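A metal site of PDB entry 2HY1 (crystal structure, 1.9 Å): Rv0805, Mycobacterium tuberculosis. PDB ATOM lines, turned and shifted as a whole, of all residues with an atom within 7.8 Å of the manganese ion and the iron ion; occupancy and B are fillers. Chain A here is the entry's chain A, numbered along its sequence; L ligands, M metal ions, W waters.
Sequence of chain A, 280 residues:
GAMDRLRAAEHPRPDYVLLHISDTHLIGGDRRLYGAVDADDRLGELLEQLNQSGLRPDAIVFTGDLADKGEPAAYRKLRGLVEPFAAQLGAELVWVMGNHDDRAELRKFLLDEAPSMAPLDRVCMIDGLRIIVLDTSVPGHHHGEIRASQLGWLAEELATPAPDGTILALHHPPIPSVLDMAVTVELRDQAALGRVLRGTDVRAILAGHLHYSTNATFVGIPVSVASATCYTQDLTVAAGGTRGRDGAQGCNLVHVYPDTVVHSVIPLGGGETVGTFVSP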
ATOM      1  N   SER A  22      11.038  24.978 -13.028  1.00  0.00           N
ATOM      2  CA  SER A  22      11.236  24.676 -11.614  1.00  0.00           C
ATOM      3  C   SER A  22      10.149  23.786 -11.062  1.00  0.00           C
ATOM      4  O   SER A  22       9.059  23.686 -11.634  1.00  0.00           O
ATOM      5  CB  SER A  22      11.292  25.969 -10.793  1.00  0.00           C
ATOM      6  OG  SER A  22      12.055  25.756  -9.617  1.00  0.00           O
ATOM      7  N   ASP A  23      10.462  23.140  -9.932  1.00  0.00           N
ATOM      8  CA  ASP A  23       9.454  22.481  -9.114  1.00  0.00           C
ATOM      9  C   ASP A  23       8.555  21.537  -9.906  1.00  0.00           C
ATOM     10  O   ASP A  23       7.319  21.680  -9.926  1.00  0.00           O
ATOM     11  CB  ASP A  23       8.650  23.543  -8.340  1.00  0.00           C
ATOM     12  CG  ASP A  23       9.493  24.269  -7.305  1.00  0.00           C
ATOM     13  OD1 ASP A  23      10.304  25.155  -7.659  1.00  0.00           O
ATOM     14  OD2 ASP A  23       9.336  23.973  -6.105  1.00  0.00           O
ATOM     15  N   THR A  24       9.175  20.568 -10.563  1.00  0.00           N
ATOM     16  CA  THR A  24       8.449  19.574 -11.362  1.00  0.00           C
ATOM     17  C   THR A  24       7.736  18.534 -10.489  1.00  0.00           C
ATOM     18  O   THR A  24       6.685  18.024 -10.864  1.00  0.00           O
ATOM     19  CB  THR A  24       9.382  18.880 -12.385  1.00  0.00           C
ATOM     20  OG1 THR A  24      10.547  18.391 -11.712  1.00  0.00           O
ATOM     21  CG2 THR A  24       9.795  19.864 -13.473  1.00  0.00           C
ATOM     22  N   HIS A  25       8.331  18.226  -9.329  1.00  0.00           N
ATOM     23  CA  HIS A  25       7.737  17.324  -8.332  1.00  0.00           C
ATOM     24  C   HIS A  25       7.265  15.968  -8.890  1.00  0.00           C
ATOM     25  O   HIS A  25       6.156  15.529  -8.605  1.00  0.00           O
ATOM     26  CB  HIS A  25       6.564  18.017  -7.602  1.00  0.00           C
ATOM     27  CG  HIS A  25       7.000  19.016  -6.579  1.00  0.00           C
ATOM     28  ND1 HIS A  25       7.048  18.725  -5.232  1.00  0.00           N
ATOM     29  CD2 HIS A  25       7.416  20.298  -6.705  1.00  0.00           C
ATOM     30  CE1 HIS A  25       7.469  19.786  -4.572  1.00  0.00           C
ATOM     31  NE2 HIS A  25       7.694  20.755  -5.435  1.00  0.00           N
ATOM     32  N   THR A  63      15.429  24.643 -11.556  1.00  0.00           N
ATOM     33  CA  THR A  63      15.844  25.172 -10.236  1.00  0.00           C
ATOM     34  C   THR A  63      15.246  24.440  -9.017  1.00  0.00           C
ATOM     35  O   THR A  63      14.787  25.064  -8.054  1.00  0.00           O
ATOM     36  CB  THR A  63      15.644  26.707 -10.113  1.00  0.00           C
ATOM     37  OG1 THR A  63      14.292  27.060 -10.409  1.00  0.00           O
ATOM     38  CG2 THR A  63      16.584  27.448 -11.070  1.00  0.00           C
ATOM     39  N   GLY A  64      15.257  23.109  -9.050  1.00  0.00           N
ATOM     40  CA  GLY A  64      15.006  22.326  -7.837  1.00  0.00           C
ATOM     41  C   GLY A  64      13.602  21.771  -7.680  1.00  0.00           C
ATOM     42  O   GLY A  64      12.699  22.113  -8.445  1.00  0.00           O
ATOM     43  N   ASP A  65      13.436  20.953  -6.639  1.00  0.00           N
ATOM     44  CA  ASP A  65      12.234  20.144  -6.408  1.00  0.00           C
ATOM     45  C   ASP A  65      11.866  19.337  -7.660  1.00  0.00           C
ATOM     46  O   ASP A  65      10.731  19.361  -8.147  1.00  0.00           O
ATOM     47  CB  ASP A  65      11.062  20.992  -5.884  1.00  0.00           C
ATOM     48  CG  ASP A  65      11.262  21.432  -4.428  1.00  0.00           C
ATOM     49  OD1 ASP A  65      12.239  20.976  -3.783  1.00  0.00           O
ATOM     50  OD2 ASP A  65      10.441  22.237  -3.941  1.00  0.00           O
ATOM     51  N   LEU A  66      12.869  18.618  -8.158  1.00  0.00           N
ATOM     52  CA  LEU A  66      12.752  17.830  -9.374  1.00  0.00           C
ATOM     53  C   LEU A  66      11.874  16.614  -9.131  1.00  0.00           C
ATOM     54  O   LEU A  66      10.975  16.327  -9.930  1.00  0.00           O
ATOM     55  CB  LEU A  66      14.137  17.428  -9.883  1.00  0.00           C
ATOM     56  CG  LEU A  66      15.228  18.509  -9.939  1.00  0.00           C
ATOM     57  CD1 LEU A  66      16.532  17.922 -10.413  1.00  0.00           C
ATOM     58  CD2 LEU A  66      14.827  19.682 -10.836  1.00  0.00           C
ATOM     59  N   ALA A  67      12.147  15.912  -8.033  1.00  0.00           N
ATOM     60  CA  ALA A  67      11.361  14.774  -7.597  1.00  0.00           C
ATOM     61  C   ALA A  67      10.684  15.111  -6.260  1.00  0.00           C
ATOM     62  O   ALA A  67      11.327  15.636  -5.351  1.00  0.00           O
ATOM     63  CB  ALA A  67      12.246  13.545  -7.450  1.00  0.00           C
ATOM     64  N   ASP A  68       9.393  14.801  -6.173  1.00  0.00           N
ATOM     65  CA  ASP A  68       8.582  15.162  -4.993  1.00  0.00           C
ATOM     66  C   ASP A  68       9.085  14.502  -3.710  1.00  0.00           C
ATOM     67  O   ASP A  68       8.994  15.105  -2.633  1.00  0.00           O
ATOM     68  CB  ASP A  68       7.112  14.824  -5.222  1.00  0.00           C
ATOM     69  CG  ASP A  68       6.222  15.275  -4.070  1.00  0.00           C
ATOM     70  OD1 ASP A  68       6.089  16.490  -3.850  1.00  0.00           O
ATOM     71  OD2 ASP A  68       5.664  14.394  -3.387  1.00  0.00           O
ATOM     72  N   MET A  97      19.465  21.196  -7.022  1.00  0.00           N
ATOM     73  CA  MET A  97      18.788  20.576  -5.885  1.00  0.00           C
ATOM     74  C   MET A  97      17.687  21.473  -5.289  1.00  0.00           C
ATOM     75  O   MET A  97      17.879  22.680  -5.145  1.00  0.00           O
ATOM     76  CB  MET A  97      19.788  20.257  -4.767  1.00  0.00           C
ATOM     77  CG  MET A  97      20.543  18.917  -4.906  1.00  0.00           C
ATOM     78  SD  MET A  97      19.520  17.462  -4.582  1.00  0.00           S
ATOM     79  CE  MET A  97      18.978  17.793  -2.910  1.00  0.00           C
ATOM     80  N   GLY A  98      16.562  20.863  -4.928  1.00  0.00           N
ATOM     81  CA  GLY A  98      15.559  21.509  -4.071  1.00  0.00           C
ATOM     82  C   GLY A  98      15.359  20.743  -2.770  1.00  0.00           C
ATOM     83  O   GLY A  98      15.930  19.659  -2.610  1.00  0.00           O
ATOM     84  N   ASN A  99      14.558  21.289  -1.856  1.00  0.00           N
ATOM     85  CA  ASN A  99      14.280  20.640  -0.563  1.00  0.00           C
ATOM     86  C   ASN A  99      13.630  19.254  -0.672  1.00  0.00           C
ATOM     87  O   ASN A  99      13.821  18.401   0.198  1.00  0.00           O
ATOM     88  CB  ASN A  99      13.463  21.542   0.382  1.00  0.00           C
ATOM     89  CG  ASN A  99      12.179  22.041  -0.244  1.00  0.00           C
ATOM     90  OD1 ASN A  99      12.201  22.715  -1.262  1.00  0.00           O
ATOM     91  ND2 ASN A  99      11.044  21.723   0.373  1.00  0.00           N
ATOM     92  N   HIS A 100      12.874  19.052  -1.745  1.00  0.00           N
ATOM     93  CA  HIS A 100      12.193  17.775  -1.972  1.00  0.00           C
ATOM     94  C   HIS A 100      13.107  16.694  -2.555  1.00  0.00           C
ATOM     95  O   HIS A 100      12.779  15.504  -2.521  1.00  0.00           O
ATOM     96  CB  HIS A 100      10.979  17.976  -2.879  1.00  0.00           C
ATOM     97  CG  HIS A 100       9.776  18.472  -2.140  1.00  0.00           C
ATOM     98  ND1 HIS A 100       8.741  17.647  -1.753  1.00  0.00           N
ATOM     99  CD2 HIS A 100       9.447  19.710  -1.718  1.00  0.00           C
ATOM    100  CE1 HIS A 100       7.830  18.359  -1.121  1.00  0.00           C
ATOM    101  NE2 HIS A 100       8.232  19.611  -1.083  1.00  0.00           N
ATOM    102  N   ASP A 101      14.257  17.114  -3.078  1.00  0.00           N
ATOM    103  CA  ASP A 101      15.191  16.189  -3.714  1.00  0.00           C
ATOM    104  C   ASP A 101      16.089  15.452  -2.725  1.00  0.00           C
ATOM    105  O   ASP A 101      16.154  15.804  -1.547  1.00  0.00           O
ATOM    106  CB  ASP A 101      16.038  16.922  -4.762  1.00  0.00           C
ATOM    107  CG  ASP A 101      15.237  17.318  -5.979  1.00  0.00           C
ATOM    108  OD1 ASP A 101      14.732  16.420  -6.693  1.00  0.00           O
ATOM    109  OD2 ASP A 101      15.112  18.535  -6.238  1.00  0.00           O
ATOM    110  N   HIS A 142      13.018  21.220   5.003  1.00  0.00           N
ATOM    111  CA  HIS A 142      12.382  21.975   3.916  1.00  0.00           C
ATOM    112  C   HIS A 142      12.897  23.417   3.750  1.00  0.00           C
ATOM    113  O   HIS A 142      12.769  24.009   2.670  1.00  0.00           O
ATOM    114  CB  HIS A 142      10.856  21.952   4.054  1.00  0.00           C
ATOM    115  CG  HIS A 142      10.263  20.599   3.835  1.00  0.00           C
ATOM    116  ND1 HIS A 142      10.345  19.936   2.622  1.00  0.00           N
ATOM    117  CD2 HIS A 142       9.578  19.771   4.666  1.00  0.00           C
ATOM    118  CE1 HIS A 142       9.738  18.767   2.716  1.00  0.00           C
ATOM    119  NE2 HIS A 142       9.262  18.653   3.946  1.00  0.00           N
ATOM    120  N   HIS A 143      13.483  23.966   4.808  1.00  0.00           N
ATOM    121  CA  HIS A 143      14.084  25.294   4.747  1.00  0.00           C
ATOM    122  C   HIS A 143      15.401  25.288   3.959  1.00  0.00           C
ATOM    123  O   HIS A 143      15.925  24.225   3.611  1.00  0.00           O
ATOM    124  CB  HIS A 143      14.291  25.871   6.158  1.00  0.00           C
ATOM    125  CG  HIS A 143      15.372  25.188   6.939  1.00  0.00           C
ATOM    126  ND1 HIS A 143      15.154  24.033   7.655  1.00  0.00           N
ATOM    127  CD2 HIS A 143      16.664  25.513   7.124  1.00  0.00           C
ATOM    128  CE1 HIS A 143      16.281  23.669   8.248  1.00  0.00           C
ATOM    129  NE2 HIS A 143      17.210  24.544   7.942  1.00  0.00           N
ATOM    130  N   HIS A 171      17.765  27.008  -5.399  1.00  0.00           N
ATOM    131  CA  HIS A 171      16.365  26.703  -5.157  1.00  0.00           C
ATOM    132  C   HIS A 171      15.641  27.747  -4.315  1.00  0.00           C
ATOM    133  O   HIS A 171      14.675  28.349  -4.775  1.00  0.00           O
ATOM    134  CB  HIS A 171      16.183  25.320  -4.546  1.00  0.00           C
ATOM    135  CG  HIS A 171      14.755  24.914  -4.403  1.00  0.00           C
ATOM    136  ND1 HIS A 171      13.926  24.677  -5.486  1.00  0.00           N
ATOM    137  CD2 HIS A 171      13.990  24.711  -3.300  1.00  0.00           C
ATOM    138  CE1 HIS A 171      12.724  24.334  -5.056  1.00  0.00           C
ATOM    139  NE2 HIS A 171      12.740  24.353  -3.732  1.00  0.00           N
ATOM    140  N   HIS A 172      16.101  27.936  -3.082  1.00  0.00           N
ATOM    141  CA  HIS A 172      15.466  28.865  -2.145  1.00  0.00           C
ATOM    142  C   HIS A 172      15.903  30.291  -2.480  1.00  0.00           C
ATOM    143  O   HIS A 172      17.087  30.619  -2.360  1.00  0.00           O
ATOM    144  CB  HIS A 172      15.861  28.535  -0.700  1.00  0.00           C
ATOM    145  CG  HIS A 172      15.415  27.187  -0.213  1.00  0.00           C
ATOM    146  ND1 HIS A 172      16.118  26.027  -0.470  1.00  0.00           N
ATOM    147  CD2 HIS A 172      14.368  26.819   0.569  1.00  0.00           C
ATOM    148  CE1 HIS A 172      15.512  25.007   0.099  1.00  0.00           C
ATOM    149  NE2 HIS A 172      14.453  25.461   0.738  1.00  0.00           N
ATOM    150  N   PRO A 173      14.945  31.164  -2.876  1.00  0.00           N
ATOM    151  CA  PRO A 173      15.292  32.531  -3.278  1.00  0.00           C
ATOM    152  C   PRO A 173      15.690  33.434  -2.105  1.00  0.00           C
ATOM    153  O   PRO A 173      15.044  33.388  -1.056  1.00  0.00           O
ATOM    154  CB  PRO A 173      14.011  33.037  -3.935  1.00  0.00           C
ATOM    155  CG  PRO A 173      12.913  32.284  -3.278  1.00  0.00           C
ATOM    156  CD  PRO A 173      13.486  30.915  -2.958  1.00  0.00           C
ATOM    157  N   VAL A 185       9.962  27.891   5.732  1.00  0.00           N
ATOM    158  CA  VAL A 185      10.750  27.132   4.761  1.00  0.00           C
ATOM    159  C   VAL A 185      11.640  28.027   3.876  1.00  0.00           C
ATOM    160  O   VAL A 185      12.134  27.585   2.832  1.00  0.00           O
ATOM    161  CB  VAL A 185       9.854  26.204   3.876  1.00  0.00           C
ATOM    162  CG1 VAL A 185       9.199  25.123   4.726  1.00  0.00           C
ATOM    163  CG2 VAL A 185       8.800  27.004   3.108  1.00  0.00           C
ATOM    164  N   GLY A 208      13.481  28.881  -7.501  1.00  0.00           N
ATOM    165  CA  GLY A 208      12.164  28.239  -7.533  1.00  0.00           C
ATOM    166  C   GLY A 208      11.545  28.325  -6.146  1.00  0.00           C
ATOM    167  O   GLY A 208      11.592  29.378  -5.507  1.00  0.00           O
ATOM    168  N   HIS A 209      10.953  27.211  -5.705  1.00  0.00           N
ATOM    169  CA  HIS A 209      10.487  27.019  -4.321  1.00  0.00           C
ATOM    170  C   HIS A 209       9.128  27.650  -4.024  1.00  0.00           C
ATOM    171  O   HIS A 209       8.312  27.041  -3.348  1.00  0.00           O
ATOM    172  CB  HIS A 209      11.549  27.505  -3.303  1.00  0.00           C
ATOM    173  CG  HIS A 209      11.267  27.122  -1.886  1.00  0.00           C
ATOM    174  ND1 HIS A 209      11.135  25.818  -1.473  1.00  0.00           N
ATOM    175  CD2 HIS A 209      11.124  27.894  -0.770  1.00  0.00           C
ATOM    176  CE1 HIS A 209      10.904  25.788  -0.171  1.00  0.00           C
ATOM    177  NE2 HIS A 209      10.896  27.038   0.276  1.00  0.00           N
ATOM    178  N   LEU A 210       8.879  28.848  -4.550  1.00  0.00           N
ATOM    179  CA  LEU A 210       7.680  29.597  -4.177  1.00  0.00           C
ATOM    180  C   LEU A 210       6.395  29.121  -4.866  1.00  0.00           C
ATOM    181  O   LEU A 210       5.300  29.324  -4.333  1.00  0.00           O
ATOM    182  CB  LEU A 210       7.890  31.103  -4.387  1.00  0.00           C
ATOM    183  CG  LEU A 210       9.058  31.753  -3.615  1.00  0.00           C
ATOM    184  CD1 LEU A 210       9.072  33.259  -3.875  1.00  0.00           C
ATOM    185  CD2 LEU A 210       8.976  31.464  -2.120  1.00  0.00           C
ATOM    186  N   HIS A 211       6.533  28.481  -6.021  1.00  0.00           N
ATOM    187  CA  HIS A 211       5.391  27.934  -6.779  1.00  0.00           C
ATOM    188  C   HIS A 211       4.460  29.022  -7.354  1.00  0.00           C
ATOM    189  O   HIS A 211       3.296  28.759  -7.659  1.00  0.00           O
ATOM    190  CB  HIS A 211       4.596  26.919  -5.943  1.00  0.00           C
ATOM    191  CG  HIS A 211       5.278  25.595  -5.770  1.00  0.00           C
ATOM    192  ND1 HIS A 211       4.688  24.404  -6.131  1.00  0.00           N
ATOM    193  CD2 HIS A 211       6.493  25.279  -5.257  1.00  0.00           C
ATOM    194  CE1 HIS A 211       5.506  23.403  -5.857  1.00  0.00           C
ATOM    195  NE2 HIS A 211       6.606  23.906  -5.330  1.00  0.00           N
ATOM    196  N   ALA A 228       5.865  26.803 -10.616  1.00  0.00           N
ATOM    197  CA  ALA A 228       5.990  25.355 -10.683  1.00  0.00           C
ATOM    198  C   ALA A 228       5.400  24.784 -11.981  1.00  0.00           C
ATOM    199  O   ALA A 228       4.585  25.431 -12.648  1.00  0.00           O
ATOM    200  CB  ALA A 228       5.316  24.705  -9.480  1.00  0.00           C
ATOM    201  N   CYS A 230       4.167  21.376 -11.868  1.00  0.00           N
ATOM    202  CA  CYS A 230       3.098  20.512 -11.354  1.00  0.00           C
ATOM    203  C   CYS A 230       1.848  21.292 -10.966  1.00  0.00           C
ATOM    204  O   CYS A 230       1.939  22.366 -10.356  1.00  0.00           O
ATOM    205  CB  CYS A 230       3.603  19.716 -10.148  1.00  0.00           C
ATOM    206  SG  CYS A 230       4.385  20.739  -8.862  1.00  0.00           S
HETATM  207  P1  LIG L   1       7.555  22.766  -1.480  1.00  0.00           P
HETATM  208  O1  LIG L   1       6.649  23.976  -1.550  1.00  0.00           O
HETATM  209  O2  LIG L   1       7.096  21.899  -0.338  1.00  0.00           O
HETATM  210  O3  LIG L   1       7.471  22.024  -2.794  1.00  0.00           O
HETATM  211  O4  LIG L   1       8.986  23.199  -1.257  1.00  0.00           O
HETATM  212 MN    MN M   1      11.037  23.903  -2.541  1.00  0.00          MN
HETATM  213 FE    FE M   2       8.500  22.767  -4.697  1.00  0.00          FE
HETATM  214  O   HOH W   1       8.986  24.297  -3.588  1.00  0.00           O
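A ring nitrogen (ND1) of His 171 lies within hydrogen-bond range of the backbone carbonyl oxygen (O) of Thr 63, at 2.7 Å.
NE2 of His 209 is in hydrogen-bond range of O of Val 185 (2.9 Å).
The backbone carbonyl oxygen (O) of His 171 is in hydrogen-bond range of the backbone NH (N) of Gly 208 (3.0 Å).
N of Asp 65 is in hydrogen-bond range of OD2 of Asp 101 (3.0 Å).
N of Thr 24 lies within hydrogen-bond range of O of Asp 65, at 3.1 Å.
The side-chain amide nitrogen of Asn 99 is in hydrogen-bond range of a ring nitrogen (ND1) of His 142 (3.0 Å).
The backbone carbonyl oxygen (O) of Leu 66 is in hydrogen-bond range of the backbone NH (N) of His 25.
The side-chain carboxylate (OD1) of Asp 65 sits at hydrogen-bond distance from the backbone NH (N) of His 100, at 2.9 Å.
Within 4 Å of the manganese ion: Asp 23, Asp 65, Asn 99, His 171 and His 209.
Along chain A the residues within 4 Å of the manganese ion span positions 23 to 209.
The nearest printed residue that does not touch the manganese ion is His 100 (4.6 Å).
Within 4 Å of the iron ion: Asp 23, His 25, Asp 65 and His 211.
Along chain A the residues within 4 Å of the iron ion span positions 23 to 211.
The manganese ion is bound by OD1 of Asn 99.
The manganese ion is bound by NE2 of His 171 (2.1 Å).
ND1 of His 209 binds the manganese ion, at 2.2 Å.
The manganese ion is bound by the side-chain carboxylate (OD2) of Asp 65, at 2.3 Å.
Water W1 binds the manganese ion.
O4 of the ligand binds the manganese ion (2.5 Å).
The manganese ion has six donor atoms within binding distance.
The iron ion is bound by water W1, OD2 of Asp 23, OD2 of Asp 65, O3 of the ligand, NE2 of His 25 and NE2 of His 211.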
